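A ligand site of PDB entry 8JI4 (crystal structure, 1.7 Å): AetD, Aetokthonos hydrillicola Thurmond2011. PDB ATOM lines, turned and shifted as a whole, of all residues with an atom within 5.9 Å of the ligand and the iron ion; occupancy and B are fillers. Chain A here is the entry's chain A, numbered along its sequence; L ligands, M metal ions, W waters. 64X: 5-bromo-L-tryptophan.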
ATOM      1  N   ILE A  51      10.026  -1.579   3.707  1.00  0.00           N
ATOM      2  CA  ILE A  51      10.696  -2.894   3.740  1.00  0.00           C
ATOM      3  C   ILE A  51      12.102  -2.782   3.102  1.00  0.00           C
ATOM      4  O   ILE A  51      12.899  -3.715   3.303  1.00  0.00           O
ATOM      5  CB  ILE A  51       9.806  -3.944   3.040  1.00  0.00           C
ATOM      6  CG1 ILE A  51       8.461  -4.015   3.778  1.00  0.00           C
ATOM      7  CG2 ILE A  51      10.527  -5.266   3.024  1.00  0.00           C
ATOM      8  CD1 ILE A  51       7.454  -4.922   3.115  1.00  0.00           C
ATOM      9  N   PHE A  54      14.915  -3.409   5.314  1.00  0.00           N
ATOM     10  CA  PHE A  54      14.962  -4.772   5.867  1.00  0.00           C
ATOM     11  C   PHE A  54      15.405  -5.825   4.799  1.00  0.00           C
ATOM     12  O   PHE A  54      16.251  -6.701   5.138  1.00  0.00           O
ATOM     13  CB  PHE A  54      13.579  -5.188   6.413  1.00  0.00           C
ATOM     14  CG  PHE A  54      13.518  -6.640   6.764  1.00  0.00           C
ATOM     15  CD1 PHE A  54      13.912  -7.095   7.992  1.00  0.00           C
ATOM     16  CD2 PHE A  54      13.122  -7.541   5.790  1.00  0.00           C
ATOM     17  CE1 PHE A  54      13.943  -8.447   8.262  1.00  0.00           C
ATOM     18  CE2 PHE A  54      13.137  -8.883   6.062  1.00  0.00           C
ATOM     19  CZ  PHE A  54      13.524  -9.342   7.305  1.00  0.00           C
ATOM     20  N   ALA A  55      14.797  -5.792   3.636  1.00  0.00           N
ATOM     21  CA  ALA A  55      14.780  -6.991   2.753  1.00  0.00           C
ATOM     22  C   ALA A  55      16.205  -7.410   2.312  1.00  0.00           C
ATOM     23  O   ALA A  55      16.497  -8.623   2.252  1.00  0.00           O
ATOM     24  CB  ALA A  55      13.879  -6.829   1.571  1.00  0.00           C
ATOM     25  N   PHE A  58      18.112  -8.817   5.132  1.00  0.00           N
ATOM     26  CA  PHE A  58      17.714 -10.201   5.428  1.00  0.00           C
ATOM     27  C   PHE A  58      18.454 -11.145   4.481  1.00  0.00           C
ATOM     28  O   PHE A  58      18.924 -12.190   4.921  1.00  0.00           O
ATOM     29  CB  PHE A  58      16.195 -10.369   5.295  1.00  0.00           C
ATOM     30  CG  PHE A  58      15.709 -11.730   5.659  1.00  0.00           C
ATOM     31  CD1 PHE A  58      15.761 -12.202   6.958  1.00  0.00           C
ATOM     32  CD2 PHE A  58      15.302 -12.588   4.658  1.00  0.00           C
ATOM     33  CE1 PHE A  58      15.287 -13.472   7.271  1.00  0.00           C
ATOM     34  CE2 PHE A  58      14.857 -13.877   4.968  1.00  0.00           C
ATOM     35  CZ  PHE A  58      14.854 -14.287   6.281  1.00  0.00           C
ATOM     36  N   ASP A  86      15.795 -18.871   1.056  1.00  0.00           N
ATOM     37  CA  ASP A  86      15.253 -17.665   1.724  1.00  0.00           C
ATOM     38  C   ASP A  86      16.043 -16.421   1.250  1.00  0.00           C
ATOM     39  O   ASP A  86      15.420 -15.361   1.207  1.00  0.00           O
ATOM     40  CB  ASP A  86      15.245 -17.869   3.234  1.00  0.00           C
ATOM     41  CG  ASP A  86      14.373 -19.052   3.677  1.00  0.00           C
ATOM     42  OD1 ASP A  86      13.521 -19.495   2.872  1.00  0.00           O
ATOM     43  OD2 ASP A  86      14.590 -19.531   4.790  1.00  0.00           O
ATOM     44  N   HIS A  89      14.699 -13.950  -1.913  1.00  0.00           N
ATOM     45  CA  HIS A  89      13.407 -13.239  -1.912  1.00  0.00           C
ATOM     46  C   HIS A  89      13.596 -11.731  -2.094  1.00  0.00           C
ATOM     47  O   HIS A  89      12.643 -11.026  -2.549  1.00  0.00           O
ATOM     48  CB  HIS A  89      12.632 -13.569  -0.629  1.00  0.00           C
ATOM     49  CG  HIS A  89      12.260 -15.022  -0.523  1.00  0.00           C
ATOM     50  ND1 HIS A  89      11.538 -15.500   0.537  1.00  0.00           N
ATOM     51  CD2 HIS A  89      12.543 -16.079  -1.314  1.00  0.00           C
ATOM     52  CE1 HIS A  89      11.369 -16.805   0.385  1.00  0.00           C
ATOM     53  NE2 HIS A  89      11.985 -17.187  -0.717  1.00  0.00           N
ATOM     54  N   TRP A  90      14.807 -11.195  -1.868  1.00  0.00           N
ATOM     55  CA  TRP A  90      15.000  -9.747  -2.037  1.00  0.00           C
ATOM     56  C   TRP A  90      14.731  -9.314  -3.473  1.00  0.00           C
ATOM     57  O   TRP A  90      14.318  -8.214  -3.706  1.00  0.00           O
ATOM     58  CB  TRP A  90      16.408  -9.386  -1.560  1.00  0.00           C
ATOM     59  CG  TRP A  90      17.478  -9.986  -2.408  1.00  0.00           C
ATOM     60  CD1 TRP A  90      17.898 -11.283  -2.407  1.00  0.00           C
ATOM     61  CD2 TRP A  90      18.218  -9.334  -3.455  1.00  0.00           C
ATOM     62  NE1 TRP A  90      18.881 -11.478  -3.345  1.00  0.00           N
ATOM     63  CE2 TRP A  90      19.089 -10.298  -4.004  1.00  0.00           C
ATOM     64  CE3 TRP A  90      18.232  -8.027  -3.959  1.00  0.00           C
ATOM     65  CZ2 TRP A  90      20.017  -9.964  -5.000  1.00  0.00           C
ATOM     66  CZ3 TRP A  90      19.106  -7.728  -4.977  1.00  0.00           C
ATOM     67  CH2 TRP A  90      19.964  -8.699  -5.483  1.00  0.00           C
ATOM     68  N   TRP A  92      12.367 -10.515  -5.401  1.00  0.00           N
ATOM     69  CA  TRP A  92      10.887 -10.400  -5.435  1.00  0.00           C
ATOM     70  C   TRP A  92      10.457  -9.055  -4.822  1.00  0.00           C
ATOM     71  O   TRP A  92       9.642  -8.363  -5.423  1.00  0.00           O
ATOM     72  CB  TRP A  92      10.222 -11.557  -4.711  1.00  0.00           C
ATOM     73  CG  TRP A  92      10.608 -12.913  -5.191  1.00  0.00           C
ATOM     74  CD1 TRP A  92      11.191 -13.241  -6.388  1.00  0.00           C
ATOM     75  CD2 TRP A  92      10.335 -14.142  -4.518  1.00  0.00           C
ATOM     76  NE1 TRP A  92      11.369 -14.605  -6.464  1.00  0.00           N
ATOM     77  CE2 TRP A  92      10.779 -15.185  -5.364  1.00  0.00           C
ATOM     78  CE3 TRP A  92       9.727 -14.479  -3.298  1.00  0.00           C
ATOM     79  CZ2 TRP A  92      10.696 -16.519  -4.987  1.00  0.00           C
ATOM     80  CZ3 TRP A  92       9.615 -15.800  -2.938  1.00  0.00           C
ATOM     81  CH2 TRP A  92      10.092 -16.816  -3.789  1.00  0.00           C
ATOM     82  N   LEU A 126      16.705  -5.031  12.658  1.00  0.00           N
ATOM     83  CA  LEU A 126      16.201  -6.364  13.060  1.00  0.00           C
ATOM     84  C   LEU A 126      17.245  -7.414  12.665  1.00  0.00           C
ATOM     85  O   LEU A 126      17.618  -8.256  13.512  1.00  0.00           O
ATOM     86  CB  LEU A 126      14.861  -6.632  12.369  1.00  0.00           C
ATOM     87  CG  LEU A 126      14.300  -8.039  12.499  1.00  0.00           C
ATOM     88  CD1 LEU A 126      14.196  -8.512  13.938  1.00  0.00           C
ATOM     89  CD2 LEU A 126      12.914  -8.070  11.860  1.00  0.00           C
ATOM     90  N   MET A 149      11.926 -16.350  13.648  1.00  0.00           N
ATOM     91  CA  MET A 149      12.014 -15.272  12.647  1.00  0.00           C
ATOM     92  C   MET A 149      11.043 -15.602  11.489  1.00  0.00           C
ATOM     93  O   MET A 149      10.306 -14.719  10.994  1.00  0.00           O
ATOM     94  CB  MET A 149      13.449 -15.099  12.177  1.00  0.00           C
ATOM     95  CG  MET A 149      13.635 -14.075  11.084  1.00  0.00           C
ATOM     96  SD  MET A 149      13.047 -12.455  11.664  1.00  0.00           S
ATOM     97  CE  MET A 149      13.665 -11.446  10.331  1.00  0.00           C
ATOM     98  N   GLU A 150      11.040 -16.856  11.087  1.00  0.00           N
ATOM     99  CA  GLU A 150      10.197 -17.313   9.947  1.00  0.00           C
ATOM    100  C   GLU A 150       8.713 -17.279  10.333  1.00  0.00           C
ATOM    101  O   GLU A 150       7.898 -16.936   9.471  1.00  0.00           O
ATOM    102  CB  GLU A 150      10.670 -18.689   9.492  1.00  0.00           C
ATOM    103  CG  GLU A 150      12.017 -18.612   8.789  1.00  0.00           C
ATOM    104  CD  GLU A 150      11.999 -17.750   7.534  1.00  0.00           C
ATOM    105  OE1 GLU A 150      11.346 -18.143   6.570  1.00  0.00           O
ATOM    106  OE2 GLU A 150      12.537 -16.620   7.560  1.00  0.00           O
ATOM    107  N   ALA A 152       7.372 -15.093  12.469  1.00  0.00           N
ATOM    108  CA  ALA A 152       7.007 -13.669  12.356  1.00  0.00           C
ATOM    109  C   ALA A 152       6.831 -13.296  10.872  1.00  0.00           C
ATOM    110  O   ALA A 152       5.888 -12.633  10.550  1.00  0.00           O
ATOM    111  CB  ALA A 152       8.003 -12.776  13.069  1.00  0.00           C
ATOM    112  N   GLY A 153       7.732 -13.702   9.991  1.00  0.00           N
ATOM    113  CA  GLY A 153       7.676 -13.404   8.534  1.00  0.00           C
ATOM    114  C   GLY A 153       6.393 -13.912   7.890  1.00  0.00           C
ATOM    115  O   GLY A 153       5.772 -13.193   7.093  1.00  0.00           O
ATOM    116  N   LEU A 154       6.014 -15.109   8.242  1.00  0.00           N
ATOM    117  CA  LEU A 154       4.793 -15.750   7.674  1.00  0.00           C
ATOM    118  C   LEU A 154       3.554 -15.008   8.117  1.00  0.00           C
ATOM    119  O   LEU A 154       2.623 -14.837   7.339  1.00  0.00           O
ATOM    120  CB  LEU A 154       4.777 -17.225   8.055  1.00  0.00           C
ATOM    121  CG  LEU A 154       5.791 -18.066   7.297  1.00  0.00           C
ATOM    122  CD1 LEU A 154       5.930 -19.450   7.917  1.00  0.00           C
ATOM    123  CD2 LEU A 154       5.401 -18.157   5.820  1.00  0.00           C
ATOM    124  N   ILE A 156       3.509 -11.719   8.659  1.00  0.00           N
ATOM    125  CA  ILE A 156       3.509 -10.485   7.891  1.00  0.00           C
ATOM    126  C   ILE A 156       3.040 -10.716   6.464  1.00  0.00           C
ATOM    127  O   ILE A 156       2.259  -9.941   5.960  1.00  0.00           O
ATOM    128  CB  ILE A 156       4.911  -9.873   7.973  1.00  0.00           C
ATOM    129  CG1 ILE A 156       5.193  -9.465   9.418  1.00  0.00           C
ATOM    130  CG2 ILE A 156       5.017  -8.734   6.963  1.00  0.00           C
ATOM    131  CD1 ILE A 156       6.667  -9.177   9.665  1.00  0.00           C
ATOM    132  N   PHE A 157       3.609 -11.709   5.831  1.00  0.00           N
ATOM    133  CA  PHE A 157       3.375 -11.962   4.396  1.00  0.00           C
ATOM    134  C   PHE A 157       2.025 -12.613   4.158  1.00  0.00           C
ATOM    135  O   PHE A 157       1.433 -12.285   3.117  1.00  0.00           O
ATOM    136  CB  PHE A 157       4.589 -12.659   3.799  1.00  0.00           C
ATOM    137  CG  PHE A 157       5.691 -11.652   3.603  1.00  0.00           C
ATOM    138  CD1 PHE A 157       5.678 -10.800   2.533  1.00  0.00           C
ATOM    139  CD2 PHE A 157       6.661 -11.508   4.574  1.00  0.00           C
ATOM    140  CE1 PHE A 157       6.694  -9.860   2.389  1.00  0.00           C
ATOM    141  CE2 PHE A 157       7.632 -10.528   4.465  1.00  0.00           C
ATOM    142  CZ  PHE A 157       7.640  -9.711   3.363  1.00  0.00           C
ATOM    143  N   TYR A 177       6.341 -10.921  -4.159  1.00  0.00           N
ATOM    144  CA  TYR A 177       6.766 -10.697  -2.762  1.00  0.00           C
ATOM    145  C   TYR A 177       5.533 -10.567  -1.865  1.00  0.00           C
ATOM    146  O   TYR A 177       5.441 -11.294  -0.900  1.00  0.00           O
ATOM    147  CB  TYR A 177       7.649  -9.443  -2.700  1.00  0.00           C
ATOM    148  CG  TYR A 177       8.422  -9.281  -1.412  1.00  0.00           C
ATOM    149  CD1 TYR A 177       9.418 -10.170  -1.028  1.00  0.00           C
ATOM    150  CD2 TYR A 177       8.183  -8.193  -0.598  1.00  0.00           C
ATOM    151  CE1 TYR A 177      10.169  -9.994   0.120  1.00  0.00           C
ATOM    152  CE2 TYR A 177       8.912  -7.988   0.561  1.00  0.00           C
ATOM    153  CZ  TYR A 177       9.890  -8.890   0.925  1.00  0.00           C
ATOM    154  OH  TYR A 177      10.634  -8.677   2.053  1.00  0.00           O
ATOM    155  N   HIS A 182       4.902 -16.399  -2.319  1.00  0.00           N
ATOM    156  CA  HIS A 182       5.965 -16.152  -1.309  1.00  0.00           C
ATOM    157  C   HIS A 182       5.640 -16.931  -0.017  1.00  0.00           C
ATOM    158  O   HIS A 182       6.522 -17.623   0.519  1.00  0.00           O
ATOM    159  CB  HIS A 182       6.090 -14.640  -1.105  1.00  0.00           C
ATOM    160  CG  HIS A 182       7.189 -14.214  -0.190  1.00  0.00           C
ATOM    161  ND1 HIS A 182       7.348 -12.874   0.172  1.00  0.00           N
ATOM    162  CD2 HIS A 182       8.179 -14.901   0.447  1.00  0.00           C
ATOM    163  CE1 HIS A 182       8.399 -12.770   0.968  1.00  0.00           C
ATOM    164  NE2 HIS A 182       8.922 -13.987   1.192  1.00  0.00           N
ATOM    165  N   GLU A 186       7.903 -20.072   1.261  1.00  0.00           N
ATOM    166  CA  GLU A 186       8.574 -19.815   2.563  1.00  0.00           C
ATOM    167  C   GLU A 186       8.267 -20.954   3.527  1.00  0.00           C
ATOM    168  O   GLU A 186       9.205 -21.449   4.186  1.00  0.00           O
ATOM    169  CB  GLU A 186       8.167 -18.476   3.173  1.00  0.00           C
ATOM    170  CG  GLU A 186       9.143 -18.040   4.268  1.00  0.00           C
ATOM    171  CD  GLU A 186      10.110 -16.957   3.826  1.00  0.00           C
ATOM    172  OE1 GLU A 186       9.805 -16.336   2.811  1.00  0.00           O
ATOM    173  OE2 GLU A 186      11.114 -16.701   4.559  1.00  0.00           O
ATOM    174  N   SER A 224      10.642  -7.916  16.096  1.00  0.00           N
ATOM    175  CA  SER A 224       9.687  -7.953  14.968  1.00  0.00           C
ATOM    176  C   SER A 224       8.514  -6.992  15.249  1.00  0.00           C
ATOM    177  O   SER A 224       8.049  -6.282  14.362  1.00  0.00           O
ATOM    178  CB  SER A 224       9.233  -9.386  14.728  1.00  0.00           C
ATOM    179  OG  SER A 224      10.315 -10.167  14.282  1.00  0.00           O
ATOM    180  N   LEU A 227       9.703  -3.399  14.620  1.00  0.00           N
ATOM    181  CA  LEU A 227       9.600  -3.174  13.161  1.00  0.00           C
ATOM    182  C   LEU A 227       8.143  -2.838  12.792  1.00  0.00           C
ATOM    183  O   LEU A 227       7.922  -1.804  12.135  1.00  0.00           O
ATOM    184  CB  LEU A 227      10.178  -4.390  12.402  1.00  0.00           C
ATOM    185  CG  LEU A 227      10.054  -4.374  10.879  1.00  0.00           C
ATOM    186  CD1 LEU A 227      11.080  -5.335  10.281  1.00  0.00           C
ATOM    187  CD2 LEU A 227       8.639  -4.770  10.416  1.00  0.00           C
ATOM    188  N   PHE A 231       6.176   0.501  10.938  1.00  0.00           N
ATOM    189  CA  PHE A 231       5.319   0.415   9.741  1.00  0.00           C
ATOM    190  C   PHE A 231       4.005   1.143  10.058  1.00  0.00           C
ATOM    191  O   PHE A 231       3.544   1.912   9.228  1.00  0.00           O
ATOM    192  CB  PHE A 231       5.105  -1.032   9.285  1.00  0.00           C
ATOM    193  CG  PHE A 231       6.257  -1.733   8.611  1.00  0.00           C
ATOM    194  CD1 PHE A 231       7.544  -1.242   8.691  1.00  0.00           C
ATOM    195  CD2 PHE A 231       6.040  -2.876   7.874  1.00  0.00           C
ATOM    196  CE1 PHE A 231       8.589  -1.904   8.066  1.00  0.00           C
ATOM    197  CE2 PHE A 231       7.087  -3.585   7.292  1.00  0.00           C
ATOM    198  CZ  PHE A 231       8.358  -3.061   7.353  1.00  0.00           C
HETATM  199  OXT 64X L   1      12.139 -10.757   2.891  1.00  0.00           O
HETATM  200  C   64X L   1      11.587 -11.918   2.917  1.00  0.00           C
HETATM  201  O   64X L   1      11.564 -12.631   1.891  1.00  0.00           O
HETATM  202  CA  64X L   1      10.791 -12.309   4.195  1.00  0.00           C
HETATM  203  N   64X L   1      10.039 -13.556   3.980  1.00  0.00           N
HETATM  204  CB  64X L   1      11.733 -12.513   5.314  1.00  0.00           C
HETATM  205  CG  64X L   1      11.208 -12.360   6.771  1.00  0.00           C
HETATM  206  CD2 64X L   1      10.707 -11.224   7.363  1.00  0.00           C
HETATM  207  CE3 64X L   1      10.370  -9.895   6.988  1.00  0.00           C
HETATM  208  CZ3 64X L   1       9.901  -8.851   7.909  1.00  0.00           C
HETATM  209 BR1  64X L   1       9.408  -7.240   7.172  1.00  0.00          BR
HETATM  210  CH2 64X L   1       9.797  -9.361   9.219  1.00  0.00           C
HETATM  211  CZ2 64X L   1      10.151 -10.647   9.614  1.00  0.00           C
HETATM  212  CE2 64X L   1      10.566 -11.566   8.666  1.00  0.00           C
HETATM  213  NE1 64X L   1      10.941 -12.794   8.880  1.00  0.00           N
HETATM  214  CD1 64X L   1      11.360 -13.332   7.694  1.00  0.00           C
HETATM  215 FE    FE M   1      10.702 -14.508   2.188  1.00  0.00          FE
HETATM  216  O   HOH W   1      12.512 -15.056   3.172  1.00  0.00           O
HETATM  217  O   HOH W   2      14.485 -10.514   1.410  1.00  0.00           O
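The side-chain hydroxyl (OH) of Tyr 177 is in hydrogen-bond range of an oxygen (OXT) of the ligand.
NE1 of the ligand lies close to SD of Met 149, 3.5 Å away.
The backbone carbonyl oxygen (O) of Met 149 sits at hydrogen-bond distance from a nitrogen (NE1) of the ligand, 2.9 Å away.
The nearest printed residue that does not touch the iron ion is Asp 86 (4.9 Å).
Residues that only touch the ligand: Phe 54 (3.1 Å), Ile 156 (3.2 Å), Gly 153 (3.3 Å), Phe 58 (3.4 Å), Glu 150 (3.5 Å) and Phe 157 (3.6 Å).
11 residues have an atom within 4 Å of the ligand: Phe 54, Phe 58, His 89, Met 149, Glu 150, Gly 153, Ile 156, Phe 157, Tyr 177, His 182 and Glu 186.
Water W2 lies within hydrogen-bond range of an oxygen (OXT) of the ligand, the backbone carbonyl oxygen (O) of Ala 55 and the backbone NH (N) of Trp 90.
The iron ion is bound by an oxygen (O) of the ligand (2.1 Å), a ring nitrogen (ND1) of His 89 (2.1 Å), a ring nitrogen (NE2) of His 182 (2.1 Å), the side-chain carboxylate (OE1) of Glu 186 (2.1 Å), water W1 (2.1 Å) and a nitrogen (N) of the ligand (2.1 Å).
The side-chain carboxylate (OE2) of Glu 186 sits close to the side-chain carboxylate (OE1) of Glu 150.
ND1 of His 182 sits at hydrogen-bond distance from O of Tyr 177 (2.7 Å).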
